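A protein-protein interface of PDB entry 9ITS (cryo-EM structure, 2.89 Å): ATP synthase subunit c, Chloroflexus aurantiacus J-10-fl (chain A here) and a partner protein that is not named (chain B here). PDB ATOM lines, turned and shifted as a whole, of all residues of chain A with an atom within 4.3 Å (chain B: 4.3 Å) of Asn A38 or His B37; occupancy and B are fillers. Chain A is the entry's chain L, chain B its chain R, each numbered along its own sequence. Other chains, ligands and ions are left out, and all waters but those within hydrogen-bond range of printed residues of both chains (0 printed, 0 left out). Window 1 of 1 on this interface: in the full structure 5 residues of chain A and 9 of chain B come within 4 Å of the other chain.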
ATOM      1  N   ALA A  34     -11.429  21.251 -11.117  1.00  0.00           N
ATOM      2  CA  ALA A  34     -12.850  21.013 -11.329  1.00  0.00           C
ATOM      3  C   ALA A  34     -13.726  22.108 -10.738  1.00  0.00           C
ATOM      4  O   ALA A  34     -14.921  22.158 -11.045  1.00  0.00           O
ATOM      5  CB  ALA A  34     -13.250  19.668 -10.728  1.00  0.00           C
ATOM      6  N   GLY A  36     -12.567  25.342 -11.032  1.00  0.00           N
ATOM      7  CA  GLY A  36     -12.368  26.423 -11.985  1.00  0.00           C
ATOM      8  C   GLY A  36     -13.447  26.460 -13.051  1.00  0.00           C
ATOM      9  O   GLY A  36     -13.851  27.533 -13.503  1.00  0.00           O
ATOM     10  N   ARG A  37     -13.925  25.291 -13.465  1.00  0.00           N
ATOM     11  CA  ARG A  37     -15.014  25.169 -14.426  1.00  0.00           C
ATOM     12  C   ARG A  37     -16.235  24.599 -13.721  1.00  0.00           C
ATOM     13  O   ARG A  37     -16.130  23.590 -13.018  1.00  0.00           O
ATOM     14  CB  ARG A  37     -14.615  24.274 -15.599  1.00  0.00           C
ATOM     15  CG  ARG A  37     -13.392  24.753 -16.359  1.00  0.00           C
ATOM     16  CD  ARG A  37     -12.822  23.647 -17.228  1.00  0.00           C
ATOM     17  NE  ARG A  37     -13.867  22.925 -17.941  1.00  0.00           N
ATOM     18  CZ  ARG A  37     -13.795  22.569 -19.216  1.00  0.00           C
ATOM     19  NH1 ARG A  37     -12.735  22.854 -19.953  1.00  0.00           N
ATOM     20  NH2 ARG A  37     -14.811  21.910 -19.765  1.00  0.00           N
ATOM     21  N   ASN A  38     -17.387  25.243 -13.917  1.00  0.00           N
ATOM     22  CA  ASN A  38     -18.645  24.912 -13.254  1.00  0.00           C
ATOM     23  C   ASN A  38     -18.509  24.954 -11.734  1.00  0.00           C
ATOM     24  O   ASN A  38     -18.548  23.902 -11.083  1.00  0.00           O
ATOM     25  CB  ASN A  38     -19.148  23.532 -13.690  1.00  0.00           C
ATOM     26  CG  ASN A  38     -19.727  23.538 -15.086  1.00  0.00           C
ATOM     27  OD1 ASN A  38     -20.365  24.503 -15.503  1.00  0.00           O
ATOM     28  ND2 ASN A  38     -19.503  22.455 -15.821  1.00  0.00           N
ATOM     29  N   PRO A  39     -18.347  26.137 -11.129  1.00  0.00           N
ATOM     30  CA  PRO A  39     -18.313  26.218  -9.662  1.00  0.00           C
ATOM     31  C   PRO A  39     -19.649  25.944  -8.989  1.00  0.00           C
ATOM     32  O   PRO A  39     -19.695  25.889  -7.756  1.00  0.00           O
ATOM     33  CB  PRO A  39     -17.856  27.662  -9.400  1.00  0.00           C
ATOM     34  CG  PRO A  39     -17.246  28.120 -10.681  1.00  0.00           C
ATOM     35  CD  PRO A  39     -18.030  27.433 -11.746  1.00  0.00           C
ATOM     36  N   GLU A  40     -20.740  25.788  -9.743  1.00  0.00           N
ATOM     37  CA  GLU A  40     -22.006  25.387  -9.143  1.00  0.00           C
ATOM     38  C   GLU A  40     -21.993  23.940  -8.668  1.00  0.00           C
ATOM     39  O   GLU A  40     -22.886  23.547  -7.910  1.00  0.00           O
ATOM     40  CB  GLU A  40     -23.151  25.598 -10.132  1.00  0.00           C
ATOM     41  CG  GLU A  40     -23.528  27.054 -10.344  1.00  0.00           C
ATOM     42  CD  GLU A  40     -25.008  27.235 -10.613  1.00  0.00           C
ATOM     43  OE1 GLU A  40     -25.709  26.217 -10.789  1.00  0.00           O
ATOM     44  OE2 GLU A  40     -25.471  28.395 -10.645  1.00  0.00           O
ATOM     45  N   ILE A  41     -21.014  23.146  -9.101  1.00  0.00           N
ATOM     46  CA  ILE A  41     -20.767  21.819  -8.550  1.00  0.00           C
ATOM     47  C   ILE A  41     -19.828  21.911  -7.343  1.00  0.00           C
ATOM     48  O   ILE A  41     -19.414  20.889  -6.781  1.00  0.00           O
ATOM     49  CB  ILE A  41     -20.230  20.891  -9.660  1.00  0.00           C
ATOM     50  CG1 ILE A  41     -21.244  20.834 -10.799  1.00  0.00           C
ATOM     51  CG2 ILE A  41     -20.113  19.432  -9.232  1.00  0.00           C
ATOM     52  CD1 ILE A  41     -22.596  20.282 -10.391  1.00  0.00           C
ATOM     53  N   GLY B  32     -21.095  19.784 -19.506  1.00  0.00           N
ATOM     54  CA  GLY B  32     -22.253  20.405 -18.895  1.00  0.00           C
ATOM     55  C   GLY B  32     -21.915  21.761 -18.312  1.00  0.00           C
ATOM     56  O   GLY B  32     -21.050  21.867 -17.440  1.00  0.00           O
ATOM     57  N   ILE B  33     -22.587  22.804 -18.783  1.00  0.00           N
ATOM     58  CA  ILE B  33     -22.268  24.173 -18.395  1.00  0.00           C
ATOM     59  C   ILE B  33     -23.279  24.651 -17.362  1.00  0.00           C
ATOM     60  O   ILE B  33     -24.493  24.540 -17.564  1.00  0.00           O
ATOM     61  CB  ILE B  33     -22.244  25.105 -19.620  1.00  0.00           C
ATOM     62  CG1 ILE B  33     -21.111  24.729 -20.581  1.00  0.00           C
ATOM     63  CG2 ILE B  33     -22.126  26.560 -19.192  1.00  0.00           C
ATOM     64  CD1 ILE B  33     -21.502  23.744 -21.667  1.00  0.00           C
ATOM     65  N   LEU B  34     -22.774  25.179 -16.253  1.00  0.00           N
ATOM     66  CA  LEU B  34     -23.555  25.734 -15.160  1.00  0.00           C
ATOM     67  C   LEU B  34     -23.464  27.254 -15.169  1.00  0.00           C
ATOM     68  O   LEU B  34     -22.535  27.825 -15.747  1.00  0.00           O
ATOM     69  CB  LEU B  34     -23.058  25.179 -13.816  1.00  0.00           C
ATOM     70  CG  LEU B  34     -23.594  23.818 -13.342  1.00  0.00           C
ATOM     71  CD1 LEU B  34     -25.096  23.886 -13.099  1.00  0.00           C
ATOM     72  CD2 LEU B  34     -23.253  22.671 -14.287  1.00  0.00           C
ATOM     73  N   PRO B  35     -24.428  27.957 -14.538  1.00  0.00           N
ATOM     74  CA  PRO B  35     -24.460  29.428 -14.634  1.00  0.00           C
ATOM     75  C   PRO B  35     -23.248  30.164 -14.073  1.00  0.00           C
ATOM     76  O   PRO B  35     -23.205  31.396 -14.121  1.00  0.00           O
ATOM     77  CB  PRO B  35     -25.719  29.809 -13.842  1.00  0.00           C
ATOM     78  CG  PRO B  35     -26.540  28.589 -13.750  1.00  0.00           C
ATOM     79  CD  PRO B  35     -25.715  27.395 -14.092  1.00  0.00           C
ATOM     80  N   ARG B  36     -22.263  29.442 -13.539  1.00  0.00           N
ATOM     81  CA  ARG B  36     -21.046  30.060 -13.027  1.00  0.00           C
ATOM     82  C   ARG B  36     -19.818  29.650 -13.836  1.00  0.00           C
ATOM     83  O   ARG B  36     -18.692  29.989 -13.454  1.00  0.00           O
ATOM     84  CB  ARG B  36     -20.874  29.705 -11.544  1.00  0.00           C
ATOM     85  CG  ARG B  36     -19.977  30.639 -10.734  1.00  0.00           C
ATOM     86  CD  ARG B  36     -20.580  32.030 -10.610  1.00  0.00           C
ATOM     87  NE  ARG B  36     -20.083  32.938 -11.635  1.00  0.00           N
ATOM     88  CZ  ARG B  36     -20.545  34.164 -11.840  1.00  0.00           C
ATOM     89  NH1 ARG B  36     -21.522  34.665 -11.100  1.00  0.00           N
ATOM     90  NH2 ARG B  36     -20.015  34.905 -12.807  1.00  0.00           N
ATOM     91  N   HIS B  37     -20.014  28.971 -14.967  1.00  0.00           N
ATOM     92  CA  HIS B  37     -18.919  28.337 -15.694  1.00  0.00           C
ATOM     93  C   HIS B  37     -17.907  29.362 -16.197  1.00  0.00           C
ATOM     94  O   HIS B  37     -18.240  30.513 -16.488  1.00  0.00           O
ATOM     95  CB  HIS B  37     -19.473  27.530 -16.870  1.00  0.00           C
ATOM     96  CG  HIS B  37     -18.457  26.671 -17.557  1.00  0.00           C
ATOM     97  ND1 HIS B  37     -17.567  27.167 -18.486  1.00  0.00           N
ATOM     98  CD2 HIS B  37     -18.195  25.347 -17.459  1.00  0.00           C
ATOM     99  CE1 HIS B  37     -16.798  26.187 -18.925  1.00  0.00           C
ATOM    100  NE2 HIS B  37     -17.159  25.072 -18.318  1.00  0.00           N
ATOM    101  N   ALA B  38     -16.651  28.922 -16.286  1.00  0.00           N
ATOM    102  CA  ALA B  38     -15.574  29.758 -16.785  1.00  0.00           C
ATOM    103  C   ALA B  38     -15.765  30.036 -18.276  1.00  0.00           C
ATOM    104  O   ALA B  38     -16.486  29.306 -18.962  1.00  0.00           O
ATOM    105  CB  ALA B  38     -14.228  29.074 -16.539  1.00  0.00           C
ATOM    106  N   PRO B  39     -15.154  31.107 -18.792  1.00  0.00           N
ATOM    107  CA  PRO B  39     -15.224  31.368 -20.237  1.00  0.00           C
ATOM    108  C   PRO B  39     -14.649  30.211 -21.042  1.00  0.00           C
ATOM    109  O   PRO B  39     -13.658  29.590 -20.654  1.00  0.00           O
ATOM    110  CB  PRO B  39     -14.390  32.641 -20.409  1.00  0.00           C
ATOM    111  CG  PRO B  39     -14.410  33.299 -19.085  1.00  0.00           C
ATOM    112  CD  PRO B  39     -14.528  32.219 -18.056  1.00  0.00           C
ATOM    113  N   LEU B  40     -15.284  29.929 -22.178  1.00  0.00           N
ATOM    114  CA  LEU B  40     -14.952  28.736 -22.943  1.00  0.00           C
ATOM    115  C   LEU B  40     -15.346  28.938 -24.399  1.00  0.00           C
ATOM    116  O   LEU B  40     -16.303  29.653 -24.703  1.00  0.00           O
ATOM    117  CB  LEU B  40     -15.661  27.505 -22.366  1.00  0.00           C
ATOM    118  CG  LEU B  40     -15.244  26.116 -22.845  1.00  0.00           C
ATOM    119  CD1 LEU B  40     -13.990  25.661 -22.123  1.00  0.00           C
ATOM    120  CD2 LEU B  40     -16.374  25.125 -22.630  1.00  0.00           C
ATOM    121  N   VAL B  69     -18.977  30.524 -24.063  1.00  0.00           N
ATOM    122  CA  VAL B  69     -19.446  30.531 -22.685  1.00  0.00           C
ATOM    123  C   VAL B  69     -18.776  31.695 -21.973  1.00  0.00           C
ATOM    124  O   VAL B  69     -17.549  31.718 -21.812  1.00  0.00           O
ATOM    125  CB  VAL B  69     -19.154  29.204 -21.974  1.00  0.00           C
ATOM    126  CG1 VAL B  69     -19.515  29.306 -20.503  1.00  0.00           C
ATOM    127  CG2 VAL B  69     -19.921  28.072 -22.636  1.00  0.00           C
ATOM    128  N   PRO B  71     -19.021  34.245 -18.356  1.00  0.00           N
ATOM    129  CA  PRO B  71     -19.442  34.047 -16.956  1.00  0.00           C
ATOM    130  C   PRO B  71     -20.888  34.424 -16.647  1.00  0.00           C
ATOM    131  O   PRO B  71     -21.380  34.042 -15.577  1.00  0.00           O
ATOM    132  CB  PRO B  71     -18.466  34.931 -16.175  1.00  0.00           C
ATOM    133  CG  PRO B  71     -17.224  34.875 -16.980  1.00  0.00           C
ATOM    134  CD  PRO B  71     -17.656  34.798 -18.427  1.00  0.00           C
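Of the 11 printed residues of chain B, 8 touch a printed residue of chain A. Hydrophobic or aromatic side chains of chain B within 4 Å of the printed part of chain A: Leu B34, Pro B35, His B37, Ala B38 and Leu B40. Along chain B the printed residues that touch a printed residue of chain A span positions 32 to 40. Printed residues of chain A that touch a printed residue of chain B: Gly A36, Arg A37, Asn A38, Pro A39 and Glu A40. Among the printed residues, 11 pairs touch across the chains.
Of chain B, only Gly B32, Ile B33, Leu B34 and His B37 come within 4 Å of Asn A38. Of the printed residues of chain A, Leu B34 touches Asn A38 and Glu A40. Of the printed residues of chain A, Pro B35 touches Glu A40. His B37 touches just these residues of chain A: Arg A37 (3.8 Å) and Asn A38 (3.0 Å). Pro B39 touches none of the printed residues of chain A. Val B69 touches none of the printed residues of chain A. The nearest printed residue of chain B that does not touch Asn A38 is Ala B38 (4.4 Å). The nearest residue of chain A that does not touch His B37 is Pro A39 (4.1 Å). The nearest printed residue of chain B that does not touch Glu A40 is His B37 (6.1 Å).
O of Gly B32 lies close to OD1 of Asn A38, at 3.3 Å. N of Leu B34 lies within hydrogen-bond range of OD1 of Asn A38 (2.6 Å).
NH2 of Arg B36 is in hydrogen-bond range of O of Pro B71 (3.2 Å). The backbone carbonyl oxygen (O) of Leu B40 lies within hydrogen-bond range of the backbone NH (N) of Val B69 (2.9 Å).
Among the printed residues, merely in contact across the chains: Asn A38 with His B37, Pro A39 with Arg B36, Glu A40 with Pro B35, Glu A40 with Leu B34, Gly A36 with Ala B38, Asn A38 with Ile B33, Arg A37 with Leu B40, Arg A37 with His B37 and Glu A40 with Arg B36.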
